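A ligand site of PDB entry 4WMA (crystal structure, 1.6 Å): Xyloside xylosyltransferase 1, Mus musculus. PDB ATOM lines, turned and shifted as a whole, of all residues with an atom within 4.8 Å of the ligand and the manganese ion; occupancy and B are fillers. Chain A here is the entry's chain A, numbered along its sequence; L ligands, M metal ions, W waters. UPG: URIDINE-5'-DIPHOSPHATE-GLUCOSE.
O of His 296 lies within hydrogen-bond range of ND2 of Asn 298. A ring nitrogen (ND1) of His 296 sits close to the side-chain amide nitrogen (ND2) of Asn 202 (3.3 Å). OE1 of Gln 244 is in hydrogen-bond range of N of Ser 203 (3.0 Å). N of Leu 27 lies within hydrogen-bond range of OD1 of Asn 24 (3.2 Å). The backbone NH (N) of Asp 243 sits at hydrogen-bond distance from the backbone carbonyl oxygen (O) of Phe 118 (3.1 Å).
Water W6 lies within hydrogen-bond range of O4' of the ligand (2.7 Å), OD1 of Asp 243 (2.8 Å) and O of Phe 118 (3.1 Å). Water W3 lies within hydrogen-bond range of the backbone carbonyl oxygen of Leu 138, an oxygen (O2C) of the ligand and the backbone NH of Met 17. Water W1 lies within hydrogen-bond range of OG of Ser 203 (3.1 Å) and O2' of the ligand (3.2 Å). Water W4 lies within hydrogen-bond range of O of His 240 (3.2 Å) and O6' of the ligand (3.3 Å). Water W2 lies within hydrogen-bond range of the side-chain amino group (NZ) of Lys 30 (3.1 Å) and an oxygen (O2A) of the ligand (3.4 Å).
Residues that only touch the ligand: Phe 18, Leu 27, Asp 243 and Asn 298. 14 residues have an atom within 4 Å of the ligand: Met 17, Phe 18, Thr 19, Leu 27, Asp 139, Leu 140, Asp 141, Ser 203, Leu 241, Asp 243, Gln 244, His 296, Asn 298 and Cys 299.
Of the 21 residues printed, 3 come within 4 Å of the manganese ion.
OE1 of Gln 244 sits at hydrogen-bond distance from O2' of the ligand (2.6 Å). O of Met 17 lies within hydrogen-bond range of O2C of the ligand (2.7 Å). N of Thr 19 sits at hydrogen-bond distance from O2 of the ligand (2.8 Å). The backbone carbonyl oxygen (O) of Thr 19 lies within hydrogen-bond range of a nitrogen (N3) of the ligand, 2.8 Å away. An oxygen (O2) of the ligand lies within hydrogen-bond range of the side-chain hydroxyl (OG1) of Thr 19, 3.3 Å away. O3C of the ligand is in hydrogen-bond range of N of Leu 140 (2.8 Å). OG of Ser 203 is in hydrogen-bond range of O3' of the ligand (2.9 Å). An oxygen (O3') of the ligand sits at hydrogen-bond distance from the backbone carbonyl oxygen (O) of Leu 241, 2.9 Å away. N of Cys 299 lies within hydrogen-bond range of O2B of the ligand, 3.0 Å away.
The manganese ion is bound by O1B of the ligand (1.9 Å), OD2 of Asp 139 (2.1 Å), NE2 of His 296 (2.2 Å), OD1 of Asp 141 (2.2 Å), OD2 of Asp 141 (2.3 Å) and O1A of the ligand (2.3 Å). The manganese ion has six donor atoms within binding distance.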
ATOM      1  N   MET A  17     -14.418  19.248  -3.207  1.00  0.00           N
ATOM      2  CA  MET A  17     -14.827  19.598  -1.848  1.00  0.00           C
ATOM      3  C   MET A  17     -13.647  19.413  -0.914  1.00  0.00           C
ATOM      4  O   MET A  17     -13.001  18.357  -0.949  1.00  0.00           O
ATOM      5  CB  MET A  17     -15.957  18.676  -1.385  1.00  0.00           C
ATOM      6  CG  MET A  17     -17.204  18.731  -2.230  1.00  0.00           C
ATOM      7  SD  MET A  17     -18.022  20.300  -1.934  1.00  0.00           S
ATOM      8  CE  MET A  17     -17.630  20.525  -0.200  1.00  0.00           C
ATOM      9  N   PHE A  18     -13.340  20.422  -0.099  1.00  0.00           N
ATOM     10  CA  PHE A  18     -12.225  20.282   0.861  1.00  0.00           C
ATOM     11  C   PHE A  18     -12.604  21.050   2.112  1.00  0.00           C
ATOM     12  O   PHE A  18     -12.285  22.230   2.252  1.00  0.00           O
ATOM     13  CB  PHE A  18     -10.895  20.774   0.252  1.00  0.00           C
ATOM     14  CG  PHE A  18      -9.675  20.475   1.079  1.00  0.00           C
ATOM     15  CD1 PHE A  18      -9.293  19.168   1.322  1.00  0.00           C
ATOM     16  CD2 PHE A  18      -8.891  21.506   1.597  1.00  0.00           C
ATOM     17  CE1 PHE A  18      -8.153  18.875   2.054  1.00  0.00           C
ATOM     18  CE2 PHE A  18      -7.748  21.227   2.332  1.00  0.00           C
ATOM     19  CZ  PHE A  18      -7.382  19.903   2.567  1.00  0.00           C
ATOM     20  N   THR A  19     -13.327  20.370   2.989  1.00  0.00           N
ATOM     21  CA  THR A  19     -13.871  20.985   4.193  1.00  0.00           C
ATOM     22  C   THR A  19     -13.412  20.264   5.443  1.00  0.00           C
ATOM     23  O   THR A  19     -13.106  19.076   5.391  1.00  0.00           O
ATOM     24  CB  THR A  19     -15.412  20.985   4.171  1.00  0.00           C
ATOM     25  OG1 THR A  19     -15.888  19.638   3.970  1.00  0.00           O
ATOM     26  CG2 THR A  19     -15.926  21.866   3.035  1.00  0.00           C
ATOM     27  N   LYS A  20     -13.371  20.988   6.552  1.00  0.00           N
ATOM     28  CA  LYS A  20     -13.011  20.391   7.867  1.00  0.00           C
ATOM     29  C   LYS A  20     -11.628  19.730   7.828  1.00  0.00           C
ATOM     30  O   LYS A  20     -11.408  18.694   8.499  1.00  0.00           O
ATOM     31  CB  LYS A  20     -14.076  19.394   8.334  1.00  0.00           C
ATOM     32  CG  LYS A  20     -15.513  19.861   8.245  1.00  0.00           C
ATOM     33  CD  LYS A  20     -15.829  20.897   9.316  1.00  0.00           C
ATOM     34  CE  LYS A  20     -17.225  21.447   9.139  1.00  0.00           C
ATOM     35  NZ  LYS A  20     -18.269  20.381   9.233  1.00  0.00           N
ATOM     36  N   ASN A  24      -7.089  17.318  10.464  1.00  0.00           N
ATOM     37  CA  ASN A  24      -7.615  16.104   9.863  1.00  0.00           C
ATOM     38  C   ASN A  24      -6.528  15.533   8.952  1.00  0.00           C
ATOM     39  O   ASN A  24      -6.545  15.725   7.730  1.00  0.00           O
ATOM     40  CB  ASN A  24      -8.920  16.377   9.089  1.00  0.00           C
ATOM     41  CG  ASN A  24      -9.584  15.112   8.566  1.00  0.00           C
ATOM     42  OD1 ASN A  24      -8.991  14.031   8.525  1.00  0.00           O
ATOM     43  ND2 ASN A  24     -10.845  15.245   8.165  1.00  0.00           N
ATOM     44  N   LEU A  27      -7.464  13.187   5.867  1.00  0.00           N
ATOM     45  CA  LEU A  27      -7.955  13.968   4.720  1.00  0.00           C
ATOM     46  C   LEU A  27      -6.862  14.733   3.983  1.00  0.00           C
ATOM     47  O   LEU A  27      -6.809  14.730   2.734  1.00  0.00           O
ATOM     48  CB  LEU A  27      -9.104  14.904   5.134  1.00  0.00           C
ATOM     49  CG  LEU A  27      -9.764  15.662   3.961  1.00  0.00           C
ATOM     50  CD1 LEU A  27     -10.475  14.698   3.027  1.00  0.00           C
ATOM     51  CD2 LEU A  27     -10.694  16.738   4.481  1.00  0.00           C
ATOM     52  N   LYS A  30      -4.823  12.284   1.902  1.00  0.00           N
ATOM     53  CA  LYS A  30      -5.563  11.900   0.701  1.00  0.00           C
ATOM     54  C   LYS A  30      -5.480  13.022  -0.335  1.00  0.00           C
ATOM     55  O   LYS A  30      -5.223  12.763  -1.521  1.00  0.00           O
ATOM     56  CB  LYS A  30      -7.025  11.601   1.031  1.00  0.00           C
ATOM     57  CG  LYS A  30      -7.241  10.335   1.847  1.00  0.00           C
ATOM     58  CD  LYS A  30      -8.657  10.324   2.403  1.00  0.00           C
ATOM     59  CE  LYS A  30      -8.942   9.047   3.177  1.00  0.00           C
ATOM     60  NZ  LYS A  30     -10.381   8.988   3.541  1.00  0.00           N
ATOM     61  N   PHE A 118     -23.658  18.445   0.363  1.00  0.00           N
ATOM     62  CA  PHE A 118     -23.532  17.125  -0.281  1.00  0.00           C
ATOM     63  C   PHE A 118     -24.363  16.973  -1.549  1.00  0.00           C
ATOM     64  O   PHE A 118     -24.219  15.968  -2.264  1.00  0.00           O
ATOM     65  CB  PHE A 118     -23.857  16.037   0.738  1.00  0.00           C
ATOM     66  CG  PHE A 118     -22.940  16.083   1.917  1.00  0.00           C
ATOM     67  CD1 PHE A 118     -21.569  15.910   1.740  1.00  0.00           C
ATOM     68  CD2 PHE A 118     -23.434  16.321   3.201  1.00  0.00           C
ATOM     69  CE1 PHE A 118     -20.703  15.963   2.825  1.00  0.00           C
ATOM     70  CE2 PHE A 118     -22.558  16.363   4.285  1.00  0.00           C
ATOM     71  CZ  PHE A 118     -21.213  16.194   4.091  1.00  0.00           C
ATOM     72  N   LEU A 138     -14.604  16.225  -8.510  1.00  0.00           N
ATOM     73  CA  LEU A 138     -13.736  15.093  -8.165  1.00  0.00           C
ATOM     74  C   LEU A 138     -13.597  14.954  -6.655  1.00  0.00           C
ATOM     75  O   LEU A 138     -13.447  15.950  -5.946  1.00  0.00           O
ATOM     76  CB  LEU A 138     -12.374  15.270  -8.824  1.00  0.00           C
ATOM     77  CG  LEU A 138     -12.361  15.269 -10.355  1.00  0.00           C
ATOM     78  CD1 LEU A 138     -11.224  16.135 -10.895  1.00  0.00           C
ATOM     79  CD2 LEU A 138     -12.285  13.848 -10.942  1.00  0.00           C
ATOM     80  N   ASP A 139     -13.673  13.716  -6.164  1.00  0.00           N
ATOM     81  CA  ASP A 139     -13.293  13.438  -4.774  1.00  0.00           C
ATOM     82  C   ASP A 139     -11.792  13.698  -4.546  1.00  0.00           C
ATOM     83  O   ASP A 139     -11.019  13.843  -5.505  1.00  0.00           O
ATOM     84  CB  ASP A 139     -13.647  11.984  -4.455  1.00  0.00           C
ATOM     85  CG  ASP A 139     -15.043  11.821  -3.904  1.00  0.00           C
ATOM     86  OD1 ASP A 139     -15.888  12.693  -4.131  1.00  0.00           O
ATOM     87  OD2 ASP A 139     -15.323  10.812  -3.240  1.00  0.00           O
ATOM     88  N   LEU A 140     -11.367  13.773  -3.280  1.00  0.00           N
ATOM     89  CA  LEU A 140      -9.951  13.956  -2.979  1.00  0.00           C
ATOM     90  C   LEU A 140      -9.241  12.681  -2.479  1.00  0.00           C
ATOM     91  O   LEU A 140      -8.060  12.710  -2.115  1.00  0.00           O
ATOM     92  CB  LEU A 140      -9.720  15.184  -2.061  1.00  0.00           C
ATOM     93  CG  LEU A 140      -9.623  16.543  -2.794  1.00  0.00           C
ATOM     94  CD1 LEU A 140      -9.805  17.768  -1.893  1.00  0.00           C
ATOM     95  CD2 LEU A 140      -8.318  16.667  -3.568  1.00  0.00           C
ATOM     96  N   ASP A 141      -9.978  11.578  -2.461  1.00  0.00           N
ATOM     97  CA  ASP A 141      -9.425  10.247  -2.130  1.00  0.00           C
ATOM     98  C   ASP A 141      -9.200   9.439  -3.414  1.00  0.00           C
ATOM     99  O   ASP A 141      -9.478   8.232  -3.460  1.00  0.00           O
ATOM    100  CB  ASP A 141     -10.331   9.521  -1.130  1.00  0.00           C
ATOM    101  CG  ASP A 141     -11.732   9.268  -1.654  1.00  0.00           C
ATOM    102  OD1 ASP A 141     -12.149   9.936  -2.633  1.00  0.00           O
ATOM    103  OD2 ASP A 141     -12.463   8.428  -1.093  1.00  0.00           O
ATOM    104  N   ASN A 202     -21.656   6.020  -8.654  1.00  0.00           N
ATOM    105  CA  ASN A 202     -20.753   6.521  -7.626  1.00  0.00           C
ATOM    106  C   ASN A 202     -20.386   7.988  -7.921  1.00  0.00           C
ATOM    107  O   ASN A 202     -20.076   8.340  -9.057  1.00  0.00           O
ATOM    108  CB  ASN A 202     -19.467   5.667  -7.621  1.00  0.00           C
ATOM    109  CG  ASN A 202     -18.517   6.034  -6.496  1.00  0.00           C
ATOM    110  OD1 ASN A 202     -18.622   5.508  -5.376  1.00  0.00           O
ATOM    111  ND2 ASN A 202     -17.600   6.952  -6.773  1.00  0.00           N
ATOM    112  N   SER A 203     -20.400   8.848  -6.886  1.00  0.00           N
ATOM    113  CA  SER A 203     -20.166  10.311  -7.116  1.00  0.00           C
ATOM    114  C   SER A 203     -18.697  10.810  -7.139  1.00  0.00           C
ATOM    115  O   SER A 203     -18.442  12.011  -7.192  1.00  0.00           O
ATOM    116  CB  SER A 203     -20.953  11.108  -6.061  1.00  0.00           C
ATOM    117  OG  SER A 203     -20.496  10.797  -4.746  1.00  0.00           O
ATOM    118  N   HIS A 240     -28.243   7.969   2.443  1.00  0.00           N
ATOM    119  CA  HIS A 240     -27.487   8.966   3.189  1.00  0.00           C
ATOM    120  C   HIS A 240     -26.233   9.418   2.487  1.00  0.00           C
ATOM    121  O   HIS A 240     -25.329   9.983   3.135  1.00  0.00           O
ATOM    122  CB  HIS A 240     -27.148   8.441   4.588  1.00  0.00           C
ATOM    123  CG  HIS A 240     -26.152   7.303   4.603  1.00  0.00           C
ATOM    124  ND1 HIS A 240     -26.516   6.022   4.400  1.00  0.00           N
ATOM    125  CD2 HIS A 240     -24.796   7.288   4.882  1.00  0.00           C
ATOM    126  CE1 HIS A 240     -25.418   5.229   4.497  1.00  0.00           C
ATOM    127  NE2 HIS A 240     -24.370   6.009   4.789  1.00  0.00           N
ATOM    128  N   LEU A 241     -26.142   9.166   1.186  1.00  0.00           N
ATOM    129  CA  LEU A 241     -24.953   9.487   0.410  1.00  0.00           C
ATOM    130  C   LEU A 241     -25.142  10.684  -0.521  1.00  0.00           C
ATOM    131  O   LEU A 241     -24.342  10.909  -1.439  1.00  0.00           O
ATOM    132  CB  LEU A 241     -24.460   8.242  -0.387  1.00  0.00           C
ATOM    133  CG  LEU A 241     -24.121   7.039   0.529  1.00  0.00           C
ATOM    134  CD1 LEU A 241     -23.672   5.851  -0.302  1.00  0.00           C
ATOM    135  CD2 LEU A 241     -23.096   7.423   1.589  1.00  0.00           C
ATOM    136  N   ASP A 243     -25.842  13.533  -3.145  1.00  0.00           N
ATOM    137  CA  ASP A 243     -25.995  13.647  -4.610  1.00  0.00           C
ATOM    138  C   ASP A 243     -25.967  12.266  -5.278  1.00  0.00           C
ATOM    139  O   ASP A 243     -26.735  11.991  -6.225  1.00  0.00           O
ATOM    140  CB  ASP A 243     -24.917  14.573  -5.212  1.00  0.00           C
ATOM    141  CG  ASP A 243     -23.474  14.159  -4.855  1.00  0.00           C
ATOM    142  OD1 ASP A 243     -23.230  13.202  -4.052  1.00  0.00           O
ATOM    143  OD2 ASP A 243     -22.567  14.803  -5.413  1.00  0.00           O
ATOM    144  N   GLN A 244     -25.142  11.390  -4.741  1.00  0.00           N
ATOM    145  CA  GLN A 244     -24.998  10.030  -5.305  1.00  0.00           C
ATOM    146  C   GLN A 244     -26.337   9.309  -5.336  1.00  0.00           C
ATOM    147  O   GLN A 244     -26.677   8.682  -6.347  1.00  0.00           O
ATOM    148  CB  GLN A 244     -23.981   9.230  -4.507  1.00  0.00           C
ATOM    149  CG  GLN A 244     -23.614   7.897  -5.183  1.00  0.00           C
ATOM    150  CD  GLN A 244     -22.565   7.170  -4.380  1.00  0.00           C
ATOM    151  OE1 GLN A 244     -21.402   7.551  -4.416  1.00  0.00           O
ATOM    152  NE2 GLN A 244     -22.973   6.120  -3.657  1.00  0.00           N
ATOM    153  N   HIS A 296      -9.976   5.054  -6.918  1.00  0.00           N
ATOM    154  CA  HIS A 296     -10.785   5.734  -5.912  1.00  0.00           C
ATOM    155  C   HIS A 296     -10.801   4.924  -4.646  1.00  0.00           C
ATOM    156  O   HIS A 296     -11.429   3.844  -4.605  1.00  0.00           O
ATOM    157  CB  HIS A 296     -12.193   5.914  -6.458  1.00  0.00           C
ATOM    158  CG  HIS A 296     -13.131   6.702  -5.555  1.00  0.00           C
ATOM    159  ND1 HIS A 296     -14.436   6.863  -5.857  1.00  0.00           N
ATOM    160  CD2 HIS A 296     -12.906   7.387  -4.364  1.00  0.00           C
ATOM    161  CE1 HIS A 296     -15.032   7.602  -4.880  1.00  0.00           C
ATOM    162  NE2 HIS A 296     -14.097   7.918  -3.970  1.00  0.00           N
ATOM    163  N   ASN A 298     -12.374   4.842  -1.815  1.00  0.00           N
ATOM    164  CA  ASN A 298     -13.551   5.161  -1.010  1.00  0.00           C
ATOM    165  C   ASN A 298     -13.681   4.292   0.235  1.00  0.00           C
ATOM    166  O   ASN A 298     -12.975   3.262   0.358  1.00  0.00           O
ATOM    167  CB  ASN A 298     -14.838   5.245  -1.876  1.00  0.00           C
ATOM    168  CG  ASN A 298     -15.220   3.944  -2.597  1.00  0.00           C
ATOM    169  OD1 ASN A 298     -16.410   3.723  -2.854  1.00  0.00           O
ATOM    170  ND2 ASN A 298     -14.245   3.144  -3.015  1.00  0.00           N
ATOM    171  N   CYS A 299     -14.532   4.722   1.176  1.00  0.00           N
ATOM    172  CA  CYS A 299     -14.599   4.199   2.554  1.00  0.00           C
ATOM    173  C   CYS A 299     -13.219   4.013   3.225  1.00  0.00           C
ATOM    174  O   CYS A 299     -12.947   2.979   3.848  1.00  0.00           O
ATOM    175  CB  CYS A 299     -15.495   2.961   2.674  1.00  0.00           C
ATOM    176  SG  CYS A 299     -14.807   1.344   2.186  1.00  0.00           S
HETATM  177  N1  UPG L   1     -14.670  15.654   2.161  1.00  0.00           N
HETATM  178  C2  UPG L   1     -14.206  16.752   2.795  1.00  0.00           C
HETATM  179  N3  UPG L   1     -14.138  16.803   4.185  1.00  0.00           N
HETATM  180  C4  UPG L   1     -14.537  15.703   4.948  1.00  0.00           C
HETATM  181  C5  UPG L   1     -15.020  14.564   4.312  1.00  0.00           C
HETATM  182  C6  UPG L   1     -15.102  14.539   2.918  1.00  0.00           C
HETATM  183  O2  UPG L   1     -13.849  17.729   2.159  1.00  0.00           O
HETATM  184  O4  UPG L   1     -14.443  15.757   6.169  1.00  0.00           O
HETATM  185  C1C UPG L   1     -14.772  15.646   0.663  1.00  0.00           C
HETATM  186  C2C UPG L   1     -13.549  15.100  -0.060  1.00  0.00           C
HETATM  187  O2C UPG L   1     -13.461  15.739  -1.360  1.00  0.00           O
HETATM  188  C3C UPG L   1     -13.933  13.635  -0.230  1.00  0.00           C
HETATM  189  C4C UPG L   1     -15.405  13.762  -0.608  1.00  0.00           C
HETATM  190  O4C UPG L   1     -15.872  14.779   0.290  1.00  0.00           O
HETATM  191  O3C UPG L   1     -13.204  13.034  -1.297  1.00  0.00           O
HETATM  192  C5C UPG L   1     -16.223  12.476  -0.323  1.00  0.00           C
HETATM  193  O5C UPG L   1     -15.832  11.848   0.920  1.00  0.00           O
HETATM  194  PA  UPG L   1     -14.866  10.593   0.836  1.00  0.00           P
HETATM  195  O1A UPG L   1     -14.073  10.622  -0.345  1.00  0.00           O
HETATM  196  O2A UPG L   1     -14.167  10.538   2.173  1.00  0.00           O
HETATM  197  O3A UPG L   1     -16.006   9.458   0.959  1.00  0.00           O
HETATM  198  PB  UPG L   1     -16.409   8.253  -0.018  1.00  0.00           P
HETATM  199  O1B UPG L   1     -15.611   8.336  -1.264  1.00  0.00           O
HETATM  200  O2B UPG L   1     -16.496   7.000   0.813  1.00  0.00           O
HETATM  201  O3B UPG L   1     -17.911   8.769  -0.402  1.00  0.00           O
HETATM  202  C1' UPG L   1     -19.167   8.290   0.099  1.00  0.00           C
HETATM  203  C2' UPG L   1     -20.288   8.451  -0.991  1.00  0.00           C
HETATM  204  C3' UPG L   1     -20.501   9.966  -1.251  1.00  0.00           C
HETATM  205  C4' UPG L   1     -20.814  10.672   0.069  1.00  0.00           C
HETATM  206  C5' UPG L   1     -19.649  10.410   1.025  1.00  0.00           C
HETATM  207  C6' UPG L   1     -19.857  11.196   2.326  1.00  0.00           C
HETATM  208  O2' UPG L   1     -19.945   7.758  -2.216  1.00  0.00           O
HETATM  209  O3' UPG L   1     -21.610  10.216  -2.179  1.00  0.00           O
HETATM  210  O4' UPG L   1     -20.913  12.093  -0.156  1.00  0.00           O
HETATM  211  O5' UPG L   1     -19.582   8.988   1.279  1.00  0.00           O
HETATM  212  O6' UPG L   1     -21.055  10.770   2.944  1.00  0.00           O
HETATM  213 MN    MN M   1     -14.224   9.281  -2.239  1.00  0.00          MN
HETATM  214  O   HOH W   1     -17.784   9.525  -3.800  1.00  0.00           O
HETATM  215  O   HOH W   2     -12.514   7.626   1.670  1.00  0.00           O
HETATM  216  O   HOH W   3     -14.767  16.478  -3.722  1.00  0.00           O
HETATM  217  O   HOH W   4     -23.701  12.516   2.130  1.00  0.00           O
HETATM  218  O   HOH W   5     -19.831   6.387   3.187  1.00  0.00           O
HETATM  219  O   HOH W   6     -21.823  14.117  -1.774  1.00  0.00           O
